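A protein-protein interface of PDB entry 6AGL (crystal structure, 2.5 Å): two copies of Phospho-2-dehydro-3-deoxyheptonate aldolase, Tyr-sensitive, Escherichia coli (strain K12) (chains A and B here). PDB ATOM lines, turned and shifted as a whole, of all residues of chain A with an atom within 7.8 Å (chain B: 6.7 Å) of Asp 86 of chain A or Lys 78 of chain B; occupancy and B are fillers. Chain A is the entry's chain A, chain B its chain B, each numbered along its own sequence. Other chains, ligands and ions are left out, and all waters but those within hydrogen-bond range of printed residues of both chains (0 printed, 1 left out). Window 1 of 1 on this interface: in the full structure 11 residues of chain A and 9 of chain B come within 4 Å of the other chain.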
ATOM      1  N   ASP A  52      -8.738 -37.283  12.641  1.00  0.00           N
ATOM      2  CA  ASP A  52      -8.648 -35.850  12.876  1.00  0.00           C
ATOM      3  C   ASP A  52      -8.294 -35.592  14.331  1.00  0.00           C
ATOM      4  O   ASP A  52      -8.955 -36.134  15.227  1.00  0.00           O
ATOM      5  CB  ASP A  52      -9.975 -35.166  12.532  1.00  0.00           C
ATOM      6  CG  ASP A  52      -9.878 -33.650  12.551  1.00  0.00           C
ATOM      7  OD1 ASP A  52      -9.973 -33.031  11.468  1.00  0.00           O
ATOM      8  OD2 ASP A  52      -9.702 -33.078  13.646  1.00  0.00           O
ATOM      9  N   PRO A  53      -7.277 -34.772  14.613  1.00  0.00           N
ATOM     10  CA  PRO A  53      -6.832 -34.615  16.006  1.00  0.00           C
ATOM     11  C   PRO A  53      -7.747 -33.747  16.854  1.00  0.00           C
ATOM     12  O   PRO A  53      -7.651 -33.807  18.085  1.00  0.00           O
ATOM     13  CB  PRO A  53      -5.447 -33.977  15.856  1.00  0.00           C
ATOM     14  CG  PRO A  53      -5.566 -33.172  14.597  1.00  0.00           C
ATOM     15  CD  PRO A  53      -6.487 -33.948  13.681  1.00  0.00           C
ATOM     16  N   ARG A  54      -8.619 -32.948  16.249  1.00  0.00           N
ATOM     17  CA  ARG A  54      -9.464 -32.045  17.019  1.00  0.00           C
ATOM     18  C   ARG A  54     -10.502 -32.816  17.829  1.00  0.00           C
ATOM     19  O   ARG A  54     -10.875 -33.945  17.497  1.00  0.00           O
ATOM     20  CB  ARG A  54     -10.154 -31.046  16.091  1.00  0.00           C
ATOM     21  CG  ARG A  54      -9.211 -30.024  15.487  1.00  0.00           C
ATOM     22  CD  ARG A  54      -9.938 -29.130  14.507  1.00  0.00           C
ATOM     23  NE  ARG A  54     -10.493 -29.896  13.399  1.00  0.00           N
ATOM     24  CZ  ARG A  54     -11.133 -29.360  12.366  1.00  0.00           C
ATOM     25  NH1 ARG A  54     -11.303 -28.046  12.299  1.00  0.00           N
ATOM     26  NH2 ARG A  54     -11.602 -30.138  11.400  1.00  0.00           N
ATOM     27  N   LEU A  55     -10.964 -32.187  18.906  1.00  0.00           N
ATOM     28  CA  LEU A  55     -11.937 -32.773  19.817  1.00  0.00           C
ATOM     29  C   LEU A  55     -13.336 -32.301  19.442  1.00  0.00           C
ATOM     30  O   LEU A  55     -13.585 -31.093  19.363  1.00  0.00           O
ATOM     31  CB  LEU A  55     -11.623 -32.383  21.263  1.00  0.00           C
ATOM     32  CG  LEU A  55     -12.431 -33.059  22.374  1.00  0.00           C
ATOM     33  CD1 LEU A  55     -11.949 -34.485  22.589  1.00  0.00           C
ATOM     34  CD2 LEU A  55     -12.356 -32.264  23.669  1.00  0.00           C
ATOM     35  N   ALA A  81     -16.377 -20.220  18.220  1.00  0.00           N
ATOM     36  CA  ALA A  81     -15.781 -21.330  17.482  1.00  0.00           C
ATOM     37  C   ALA A  81     -14.623 -20.871  16.609  1.00  0.00           C
ATOM     38  O   ALA A  81     -13.650 -21.613  16.428  1.00  0.00           O
ATOM     39  CB  ALA A  81     -16.842 -22.023  16.626  1.00  0.00           C
ATOM     40  N   ALA A  82     -14.707 -19.658  16.058  1.00  0.00           N
ATOM     41  CA  ALA A  82     -13.619 -19.123  15.247  1.00  0.00           C
ATOM     42  C   ALA A  82     -12.342 -18.924  16.051  1.00  0.00           C
ATOM     43  O   ALA A  82     -11.265 -18.793  15.460  1.00  0.00           O
ATOM     44  CB  ALA A  82     -14.044 -17.799  14.609  1.00  0.00           C
ATOM     45  N   GLU A  83     -12.436 -18.893  17.382  1.00  0.00           N
ATOM     46  CA  GLU A  83     -11.289 -18.655  18.246  1.00  0.00           C
ATOM     47  C   GLU A  83     -10.744 -19.920  18.898  1.00  0.00           C
ATOM     48  O   GLU A  83      -9.631 -19.890  19.436  1.00  0.00           O
ATOM     49  CB  GLU A  83     -11.657 -17.641  19.338  1.00  0.00           C
ATOM     50  CG  GLU A  83     -11.899 -16.230  18.820  1.00  0.00           C
ATOM     51  CD  GLU A  83     -12.366 -15.279  19.907  1.00  0.00           C
ATOM     52  OE1 GLU A  83     -13.279 -14.467  19.636  1.00  0.00           O
ATOM     53  OE2 GLU A  83     -11.826 -15.347  21.032  1.00  0.00           O
ATOM     54  N   VAL A  84     -11.492 -21.020  18.875  1.00  0.00           N
ATOM     55  CA  VAL A  84     -11.032 -22.290  19.420  1.00  0.00           C
ATOM     56  C   VAL A  84     -10.962 -23.364  18.337  1.00  0.00           C
ATOM     57  O   VAL A  84     -10.906 -24.551  18.640  1.00  0.00           O
ATOM     58  CB  VAL A  84     -11.919 -22.746  20.594  1.00  0.00           C
ATOM     59  CG1 VAL A  84     -11.786 -21.785  21.765  1.00  0.00           C
ATOM     60  CG2 VAL A  84     -13.370 -22.859  20.148  1.00  0.00           C
ATOM     61  N   SER A  85     -10.955 -22.951  17.067  1.00  0.00           N
ATOM     62  CA  SER A  85     -11.051 -23.896  15.961  1.00  0.00           C
ATOM     63  C   SER A  85      -9.816 -24.777  15.823  1.00  0.00           C
ATOM     64  O   SER A  85      -9.906 -25.852  15.223  1.00  0.00           O
ATOM     65  CB  SER A  85     -11.289 -23.144  14.650  1.00  0.00           C
ATOM     66  OG  SER A  85     -10.160 -22.359  14.304  1.00  0.00           O
ATOM     67  N   ASP A  86      -8.670 -24.351  16.358  1.00  0.00           N
ATOM     68  CA  ASP A  86      -7.452 -25.140  16.201  1.00  0.00           C
ATOM     69  C   ASP A  86      -7.542 -26.464  16.952  1.00  0.00           C
ATOM     70  O   ASP A  86      -7.108 -27.502  16.443  1.00  0.00           O
ATOM     71  CB  ASP A  86      -6.237 -24.339  16.671  1.00  0.00           C
ATOM     72  CG  ASP A  86      -6.412 -23.781  18.069  1.00  0.00           C
ATOM     73  OD1 ASP A  86      -7.489 -23.213  18.351  1.00  0.00           O
ATOM     74  OD2 ASP A  86      -5.477 -23.914  18.890  1.00  0.00           O
ATOM     75  N   SER A  87      -8.107 -26.450  18.158  1.00  0.00           N
ATOM     76  CA  SER A  87      -8.179 -27.648  18.986  1.00  0.00           C
ATOM     77  C   SER A  87      -9.560 -28.284  19.019  1.00  0.00           C
ATOM     78  O   SER A  87      -9.659 -29.512  19.120  1.00  0.00           O
ATOM     79  CB  SER A  87      -7.749 -27.326  20.422  1.00  0.00           C
ATOM     80  OG  SER A  87      -6.430 -26.815  20.461  1.00  0.00           O
ATOM     81  N   LEU A  88     -10.625 -27.490  18.936  1.00  0.00           N
ATOM     82  CA  LEU A  88     -11.983 -27.971  19.133  1.00  0.00           C
ATOM     83  C   LEU A  88     -12.821 -27.754  17.879  1.00  0.00           C
ATOM     84  O   LEU A  88     -12.634 -26.779  17.145  1.00  0.00           O
ATOM     85  CB  LEU A  88     -12.653 -27.264  20.315  1.00  0.00           C
ATOM     86  CG  LEU A  88     -11.886 -27.282  21.637  1.00  0.00           C
ATOM     87  CD1 LEU A  88     -12.666 -26.539  22.706  1.00  0.00           C
ATOM     88  CD2 LEU A  88     -11.605 -28.708  22.066  1.00  0.00           C
ATOM     89  N   TYR A  89     -13.758 -28.673  17.652  1.00  0.00           N
ATOM     90  CA  TYR A  89     -14.693 -28.608  16.534  1.00  0.00           C
ATOM     91  C   TYR A  89     -16.093 -28.433  17.110  1.00  0.00           C
ATOM     92  O   TYR A  89     -16.666 -29.383  17.652  1.00  0.00           O
ATOM     93  CB  TYR A  89     -14.606 -29.863  15.668  1.00  0.00           C
ATOM     94  CG  TYR A  89     -15.249 -29.704  14.309  1.00  0.00           C
ATOM     95  CD1 TYR A  89     -14.519 -29.232  13.226  1.00  0.00           C
ATOM     96  CD2 TYR A  89     -16.587 -30.019  14.109  1.00  0.00           C
ATOM     97  CE1 TYR A  89     -15.101 -29.080  11.984  1.00  0.00           C
ATOM     98  CE2 TYR A  89     -17.178 -29.872  12.868  1.00  0.00           C
ATOM     99  CZ  TYR A  89     -16.430 -29.402  11.812  1.00  0.00           C
ATOM    100  OH  TYR A  89     -17.015 -29.251  10.576  1.00  0.00           O
ATOM    101  N   HIS A 344      -9.605 -25.317  25.548  1.00  0.00           N
ATOM    102  CA  HIS A 344      -8.714 -24.970  24.447  1.00  0.00           C
ATOM    103  C   HIS A 344      -7.298 -24.691  24.941  1.00  0.00           C
ATOM    104  O   HIS A 344      -6.320 -25.134  24.328  1.00  0.00           O
ATOM    105  CB  HIS A 344      -9.272 -23.762  23.697  1.00  0.00           C
ATOM    106  CG  HIS A 344      -8.358 -23.229  22.641  1.00  0.00           C
ATOM    107  ND1 HIS A 344      -7.421 -22.251  22.893  1.00  0.00           N
ATOM    108  CD2 HIS A 344      -8.239 -23.534  21.327  1.00  0.00           C
ATOM    109  CE1 HIS A 344      -6.763 -21.976  21.781  1.00  0.00           C
ATOM    110  NE2 HIS A 344      -7.241 -22.740  20.816  1.00  0.00           N
ATOM    111  N   GLN A 345      -7.171 -23.967  26.055  1.00  0.00           N
ATOM    112  CA  GLN A 345      -5.848 -23.603  26.552  1.00  0.00           C
ATOM    113  C   GLN A 345      -5.120 -24.798  27.157  1.00  0.00           C
ATOM    114  O   GLN A 345      -3.885 -24.833  27.150  1.00  0.00           O
ATOM    115  CB  GLN A 345      -5.960 -22.480  27.587  1.00  0.00           C
ATOM    116  CG  GLN A 345      -6.439 -21.156  27.018  1.00  0.00           C
ATOM    117  CD  GLN A 345      -6.608 -20.091  28.081  1.00  0.00           C
ATOM    118  OE1 GLN A 345      -6.818 -20.403  29.254  1.00  0.00           O
ATOM    119  NE2 GLN A 345      -6.514 -18.828  27.676  1.00  0.00           N
ATOM    120  N   LEU A 347      -5.638 -28.122  26.148  1.00  0.00           N
ATOM    121  CA  LEU A 347      -5.394 -29.136  25.127  1.00  0.00           C
ATOM    122  C   LEU A 347      -4.275 -28.769  24.162  1.00  0.00           C
ATOM    123  O   LEU A 347      -4.070 -29.500  23.186  1.00  0.00           O
ATOM    124  CB  LEU A 347      -6.667 -29.399  24.316  1.00  0.00           C
ATOM    125  CG  LEU A 347      -7.814 -30.155  24.981  1.00  0.00           C
ATOM    126  CD1 LEU A 347      -8.921 -30.410  23.968  1.00  0.00           C
ATOM    127  CD2 LEU A 347      -7.328 -31.457  25.592  1.00  0.00           C
ATOM    128  N   ASN A 348      -3.569 -27.659  24.389  1.00  0.00           N
ATOM    129  CA  ASN A 348      -2.579 -27.188  23.423  1.00  0.00           C
ATOM    130  C   ASN A 348      -1.526 -28.250  23.127  1.00  0.00           C
ATOM    131  O   ASN A 348      -1.256 -28.566  21.962  1.00  0.00           O
ATOM    132  CB  ASN A 348      -1.926 -25.901  23.930  1.00  0.00           C
ATOM    133  CG  ASN A 348      -1.526 -25.985  25.390  1.00  0.00           C
ATOM    134  OD1 ASN A 348      -1.638 -27.039  26.020  1.00  0.00           O
ATOM    135  ND2 ASN A 348      -1.050 -24.872  25.936  1.00  0.00           N
ATOM    136  N   GLN A 350      -0.603 -31.471  22.228  1.00  0.00           N
ATOM    137  CA  GLN A 350      -1.197 -32.655  21.602  1.00  0.00           C
ATOM    138  C   GLN A 350      -1.289 -32.421  20.095  1.00  0.00           C
ATOM    139  O   GLN A 350      -0.406 -32.817  19.334  1.00  0.00           O
ATOM    140  CB  GLN A 350      -2.588 -32.976  22.162  1.00  0.00           C
ATOM    141  CG  GLN A 350      -3.195 -34.261  21.621  1.00  0.00           C
ATOM    142  CD  GLN A 350      -4.013 -34.027  20.368  1.00  0.00           C
ATOM    143  OE1 GLN A 350      -4.823 -33.103  20.310  1.00  0.00           O
ATOM    144  NE2 GLN A 350      -3.798 -34.857  19.353  1.00  0.00           N
ATOM    145  N   TYR B  73      -3.722 -16.424  12.916  1.00  0.00           N
ATOM    146  CA  TYR B  73      -3.466 -17.088  11.647  1.00  0.00           C
ATOM    147  C   TYR B  73      -3.084 -18.546  11.860  1.00  0.00           C
ATOM    148  O   TYR B  73      -3.488 -19.415  11.084  1.00  0.00           O
ATOM    149  CB  TYR B  73      -2.368 -16.354  10.879  1.00  0.00           C
ATOM    150  CG  TYR B  73      -2.147 -16.911   9.494  1.00  0.00           C
ATOM    151  CD1 TYR B  73      -2.856 -16.416   8.408  1.00  0.00           C
ATOM    152  CD2 TYR B  73      -1.243 -17.942   9.273  1.00  0.00           C
ATOM    153  CE1 TYR B  73      -2.667 -16.928   7.143  1.00  0.00           C
ATOM    154  CE2 TYR B  73      -1.049 -18.461   8.011  1.00  0.00           C
ATOM    155  CZ  TYR B  73      -1.761 -17.948   6.949  1.00  0.00           C
ATOM    156  OH  TYR B  73      -1.570 -18.459   5.686  1.00  0.00           O
ATOM    157  N   ALA B  74      -2.321 -18.834  12.917  1.00  0.00           N
ATOM    158  CA  ALA B  74      -1.878 -20.200  13.172  1.00  0.00           C
ATOM    159  C   ALA B  74      -3.030 -21.085  13.627  1.00  0.00           C
ATOM    160  O   ALA B  74      -3.073 -22.269  13.288  1.00  0.00           O
ATOM    161  CB  ALA B  74      -0.760 -20.201  14.209  1.00  0.00           C
ATOM    162  N   ARG B  75      -3.965 -20.535  14.404  1.00  0.00           N
ATOM    163  CA  ARG B  75      -5.149 -21.304  14.780  1.00  0.00           C
ATOM    164  C   ARG B  75      -5.971 -21.664  13.550  1.00  0.00           C
ATOM    165  O   ARG B  75      -6.383 -22.819  13.375  1.00  0.00           O
ATOM    166  CB  ARG B  75      -5.999 -20.522  15.782  1.00  0.00           C
ATOM    167  CG  ARG B  75      -5.316 -20.259  17.107  1.00  0.00           C
ATOM    168  CD  ARG B  75      -6.280 -19.653  18.112  1.00  0.00           C
ATOM    169  NE  ARG B  75      -5.611 -18.695  18.986  1.00  0.00           N
ATOM    170  CZ  ARG B  75      -5.715 -17.376  18.863  1.00  0.00           C
ATOM    171  NH1 ARG B  75      -5.067 -16.574  19.697  1.00  0.00           N
ATOM    172  NH2 ARG B  75      -6.478 -16.859  17.911  1.00  0.00           N
ATOM    173  N   ARG B  76      -6.209 -20.682  12.675  1.00  0.00           N
ATOM    174  CA  ARG B  76      -6.940 -20.975  11.442  1.00  0.00           C
ATOM    175  C   ARG B  76      -6.180 -21.976  10.573  1.00  0.00           C
ATOM    176  O   ARG B  76      -6.778 -22.889   9.988  1.00  0.00           O
ATOM    177  CB  ARG B  76      -7.204 -19.684  10.671  1.00  0.00           C
ATOM    178  CG  ARG B  76      -8.024 -18.666  11.438  1.00  0.00           C
ATOM    179  CD  ARG B  76      -8.336 -17.461  10.572  1.00  0.00           C
ATOM    180  NE  ARG B  76      -9.023 -16.411  11.318  1.00  0.00           N
ATOM    181  CZ  ARG B  76      -9.446 -15.272  10.781  1.00  0.00           C
ATOM    182  NH1 ARG B  76      -9.256 -15.037   9.491  1.00  0.00           N
ATOM    183  NH2 ARG B  76     -10.061 -14.368  11.533  1.00  0.00           N
ATOM    184  N   PHE B  77      -4.857 -21.828  10.499  1.00  0.00           N
ATOM    185  CA  PHE B  77      -4.027 -22.702   9.680  1.00  0.00           C
ATOM    186  C   PHE B  77      -4.039 -24.132  10.207  1.00  0.00           C
ATOM    187  O   PHE B  77      -4.089 -25.089   9.426  1.00  0.00           O
ATOM    188  CB  PHE B  77      -2.604 -22.142   9.648  1.00  0.00           C
ATOM    189  CG  PHE B  77      -1.723 -22.752   8.602  1.00  0.00           C
ATOM    190  CD1 PHE B  77      -1.866 -22.406   7.268  1.00  0.00           C
ATOM    191  CD2 PHE B  77      -0.725 -23.643   8.955  1.00  0.00           C
ATOM    192  CE1 PHE B  77      -1.045 -22.956   6.304  1.00  0.00           C
ATOM    193  CE2 PHE B  77       0.100 -24.195   7.998  1.00  0.00           C
ATOM    194  CZ  PHE B  77      -0.061 -23.850   6.671  1.00  0.00           C
ATOM    195  N   LYS B  78      -3.990 -24.293  11.529  1.00  0.00           N
ATOM    196  CA  LYS B  78      -4.046 -25.621  12.130  1.00  0.00           C
ATOM    197  C   LYS B  78      -5.412 -26.257  11.922  1.00  0.00           C
ATOM    198  O   LYS B  78      -5.507 -27.455  11.628  1.00  0.00           O
ATOM    199  CB  LYS B  78      -3.709 -25.530  13.619  1.00  0.00           C
ATOM    200  CG  LYS B  78      -3.853 -26.831  14.387  1.00  0.00           C
ATOM    201  CD  LYS B  78      -2.690 -27.772  14.129  1.00  0.00           C
ATOM    202  CE  LYS B  78      -2.789 -28.990  15.026  1.00  0.00           C
ATOM    203  NZ  LYS B  78      -2.817 -28.594  16.463  1.00  0.00           N
ATOM    204  N   ALA B  79      -6.484 -25.471  12.065  1.00  0.00           N
ATOM    205  CA  ALA B  79      -7.816 -26.002  11.799  1.00  0.00           C
ATOM    206  C   ALA B  79      -7.952 -26.450  10.348  1.00  0.00           C
ATOM    207  O   ALA B  79      -8.610 -27.456  10.059  1.00  0.00           O
ATOM    208  CB  ALA B  79      -8.878 -24.958  12.144  1.00  0.00           C
ATOM    209  N   LEU B  80      -7.331 -25.718   9.420  1.00  0.00           N
ATOM    210  CA  LEU B  80      -7.411 -26.098   8.013  1.00  0.00           C
ATOM    211  C   LEU B  80      -6.559 -27.328   7.713  1.00  0.00           C
ATOM    212  O   LEU B  80      -6.979 -28.211   6.955  1.00  0.00           O
ATOM    213  CB  LEU B  80      -6.991 -24.928   7.124  1.00  0.00           C
ATOM    214  CG  LEU B  80      -6.989 -25.193   5.619  1.00  0.00           C
ATOM    215  CD1 LEU B  80      -8.346 -25.701   5.151  1.00  0.00           C
ATOM    216  CD2 LEU B  80      -6.605 -23.929   4.876  1.00  0.00           C
ATOM    217  N   ALA B  81      -5.357 -27.401   8.294  1.00  0.00           N
ATOM    218  CA  ALA B  81      -4.459 -28.519   8.023  1.00  0.00           C
ATOM    219  C   ALA B  81      -5.046 -29.843   8.493  1.00  0.00           C
ATOM    220  O   ALA B  81      -4.793 -30.886   7.879  1.00  0.00           O
ATOM    221  CB  ALA B  81      -3.105 -28.280   8.689  1.00  0.00           C
ATOM    222  N   ALA B  82      -5.825 -29.821   9.577  1.00  0.00           N
ATOM    223  CA  ALA B  82      -6.461 -31.039  10.063  1.00  0.00           C
ATOM    224  C   ALA B  82      -7.477 -31.591   9.071  1.00  0.00           C
ATOM    225  O   ALA B  82      -7.861 -32.761   9.180  1.00  0.00           O
ATOM    226  CB  ALA B  82      -7.137 -30.779  11.411  1.00  0.00           C
ATOM    227  N   GLU B  83      -7.919 -30.781   8.109  1.00  0.00           N
ATOM    228  CA  GLU B  83      -8.920 -31.198   7.138  1.00  0.00           C
ATOM    229  C   GLU B  83      -8.339 -31.535   5.771  1.00  0.00           C
ATOM    230  O   GLU B  83      -9.027 -32.169   4.964  1.00  0.00           O
ATOM    231  CB  GLU B  83      -9.987 -30.110   6.986  1.00  0.00           C
ATOM    232  CG  GLU B  83     -10.876 -29.974   8.211  1.00  0.00           C
ATOM    233  CD  GLU B  83     -11.851 -28.820   8.108  1.00  0.00           C
ATOM    234  OE1 GLU B  83     -12.009 -28.080   9.104  1.00  0.00           O
ATOM    235  OE2 GLU B  83     -12.456 -28.651   7.028  1.00  0.00           O
ATOM    236  N   LEU B  90       0.894 -29.195   5.515  1.00  0.00           N
ATOM    237  CA  LEU B  90       0.929 -27.747   5.670  1.00  0.00           C
ATOM    238  C   LEU B  90       2.058 -27.330   6.603  1.00  0.00           C
ATOM    239  O   LEU B  90       2.185 -27.855   7.715  1.00  0.00           O
ATOM    240  CB  LEU B  90      -0.410 -27.232   6.200  1.00  0.00           C
ATOM    241  CG  LEU B  90      -1.627 -27.401   5.288  1.00  0.00           C
ATOM    242  CD1 LEU B  90      -2.704 -26.384   5.632  1.00  0.00           C
ATOM    243  CD2 LEU B  90      -1.238 -27.287   3.828  1.00  0.00           C
ATOM    244  N   ASN B 136       4.164 -25.511  19.988  1.00  0.00           N
ATOM    245  CA  ASN B 136       3.301 -26.152  20.976  1.00  0.00           C
ATOM    246  C   ASN B 136       1.918 -26.451  20.409  1.00  0.00           C
ATOM    247  O   ASN B 136       1.270 -27.415  20.833  1.00  0.00           O
ATOM    248  CB  ASN B 136       3.192 -25.266  22.218  1.00  0.00           C
ATOM    249  CG  ASN B 136       2.489 -25.956  23.369  1.00  0.00           C
ATOM    250  OD1 ASN B 136       2.497 -27.182  23.476  1.00  0.00           O
ATOM    251  ND2 ASN B 136       1.875 -25.166  24.243  1.00  0.00           N
ATOM    252  N   MET B 137       1.453 -25.648  19.449  1.00  0.00           N
ATOM    253  CA  MET B 137       0.197 -25.940  18.769  1.00  0.00           C
ATOM    254  C   MET B 137       0.299 -27.132  17.830  1.00  0.00           C
ATOM    255  O   MET B 137      -0.720 -27.531  17.254  1.00  0.00           O
ATOM    256  CB  MET B 137      -0.276 -24.716  17.984  1.00  0.00           C
ATOM    257  CG  MET B 137      -0.631 -23.512  18.839  1.00  0.00           C
ATOM    258  SD  MET B 137      -1.095 -22.085  17.836  1.00  0.00           S
ATOM    259  CE  MET B 137      -2.479 -22.755  16.918  1.00  0.00           C
ATOM    260  N   GLY B 138       1.485 -27.715  17.673  1.00  0.00           N
ATOM    261  CA  GLY B 138       1.677 -28.822  16.759  1.00  0.00           C
ATOM    262  C   GLY B 138       1.686 -28.377  15.312  1.00  0.00           C
ATOM    263  O   GLY B 138       1.002 -28.963  14.468  1.00  0.00           O
ATOM    264  N   LEU B 139       2.461 -27.337  15.017  1.00  0.00           N
ATOM    265  CA  LEU B 139       2.540 -26.760  13.682  1.00  0.00           C
ATOM    266  C   LEU B 139       3.990 -26.754  13.216  1.00  0.00           C
ATOM    267  O   LEU B 139       4.845 -26.144  13.882  1.00  0.00           O
ATOM    268  CB  LEU B 139       1.972 -25.338  13.669  1.00  0.00           C
ATOM    269  CG  LEU B 139       0.455 -25.180  13.558  1.00  0.00           C
ATOM    270  CD1 LEU B 139       0.033 -23.813  14.065  1.00  0.00           C
ATOM    271  CD2 LEU B 139       0.009 -25.374  12.118  1.00  0.00           C
ATOM    272  N   TRP B 333      -7.377 -14.777   3.756  1.00  0.00           N
ATOM    273  CA  TRP B 333      -7.545 -16.098   4.348  1.00  0.00           C
ATOM    274  C   TRP B 333      -8.708 -16.858   3.721  1.00  0.00           C
ATOM    275  O   TRP B 333      -8.659 -18.088   3.631  1.00  0.00           O
ATOM    276  CB  TRP B 333      -7.742 -15.996   5.859  1.00  0.00           C
ATOM    277  CG  TRP B 333      -8.084 -17.321   6.448  1.00  0.00           C
ATOM    278  CD1 TRP B 333      -9.294 -17.713   6.938  1.00  0.00           C
ATOM    279  CD2 TRP B 333      -7.216 -18.456   6.561  1.00  0.00           C
ATOM    280  NE1 TRP B 333      -9.228 -19.016   7.370  1.00  0.00           N
ATOM    281  CE2 TRP B 333      -7.963 -19.494   7.148  1.00  0.00           C
ATOM    282  CE3 TRP B 333      -5.877 -18.689   6.231  1.00  0.00           C
ATOM    283  CZ2 TRP B 333      -7.417 -20.748   7.413  1.00  0.00           C
ATOM    284  CZ3 TRP B 333      -5.335 -19.935   6.495  1.00  0.00           C
ATOM    285  CH2 TRP B 333      -6.104 -20.948   7.081  1.00  0.00           C
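Positions printed for both chains: 81, 82 and 83.
The guanidinium group (NH2) of Arg 54 of chain A is in salt-bridge range of the side-chain carboxylate (OE1) of Glu 83 of chain B (3.1 Å).
ND2 of Asn 348 of chain A lies close to ND2 of Asn 136 of chain B.
The backbone carbonyl oxygen (O) of Ala 82 of chain B lies close to the side-chain carboxylate (OD1) of Asp 52 of chain A.
The side-chain carboxylate (OD2) of Asp 52 of chain A is in salt-bridge range of the guanidinium group (NE) of Arg 54 of chain A, at 3.3 Å.
OG of Ser 87 of chain A sits at hydrogen-bond distance from OD2 of Asp 86 of chain A, 3.4 Å away.
NE2 of His 344 of chain A sits at hydrogen-bond distance from OD1 of Asp 86 of chain A (2.5 Å).
The backbone carbonyl oxygen of Gln 345 of chain A sits at hydrogen-bond distance from the side-chain amide nitrogen of Asn 348 of chain A (3.1 Å).
The backbone carbonyl oxygen (O) of Met 137 of chain B sits at hydrogen-bond distance from the side-chain amino group (NZ) of Lys 78 of chain B, 2.5 Å away.
Of the 17 printed residues of chain B, 7 touch a printed residue of chain A.
Hydrophobic or aromatic side chains of chain B within 4 Å of the printed part of chain A: Ala 79, Ala 82 and Met 137.
Along chain B the printed residues that touch a printed residue of chain A span positions 75 to 137.
Of the 18 printed residues of chain A, 7 touch a printed residue of chain B.
Printed residues of chain A that touch a printed residue of chain B: Asp 52, Pro 53, Arg 54, Glu 83, Ser 85, Asp 86 and Asn 348.
Among the printed residues, 12 pairs touch across the chains.
Pro 53 of chain A touches Ala 82 of chain B (CD to CB, 3.95 Å).
Ala 79 of chain B touches Arg 54 of chain A.
NE of Arg 54 of chain A touches CB of Ala 82 of chain B, at 3.999 Å.
Glu 83 of chain A touches Arg 75 of chain B (O to CD, 3.6 Å).
Ser 85 of chain A touches Arg 75 of chain B.
O of Ser 85 of chain A touches CB of Ala 79 of chain B, at 3.4 Å.
CB of Asp 86 of chain A touches O of Arg 75 of chain B (3.6 Å).
Asp 86 of chain A touches Lys 78 of chain B.
CE of Met 137 of chain B touches OD2 of Asp 86 of chain A, 3.8 Å away.
Of chain B, only Arg 75 (3.6 Å), Lys 78 (3.9 Å) and Met 137 (3.8 Å) come within 4 Å of Asp 86 of chain A.
Lys 78 of chain B touches just one residue of chain A: Asp 86.
Of the printed residues of chain B, Asn 348 of chain A touches Asn 136.
Of the printed residues of chain B, Arg 54 of chain A touches Ala 79, Ala 82 and Glu 83.
Of the printed residues of chain B, Pro 53 of chain A touches Ala 82.
Printed residues of chain B within 4 Å of Glu 83 of chain A: Arg 75.
The nearest residue of chain B that does not touch Asp 86 of chain A is Ala 79 of chain B (4.3 Å).
The nearest residue of chain A that does not touch Lys 78 of chain B is Pro 53 of chain A (5.0 Å).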
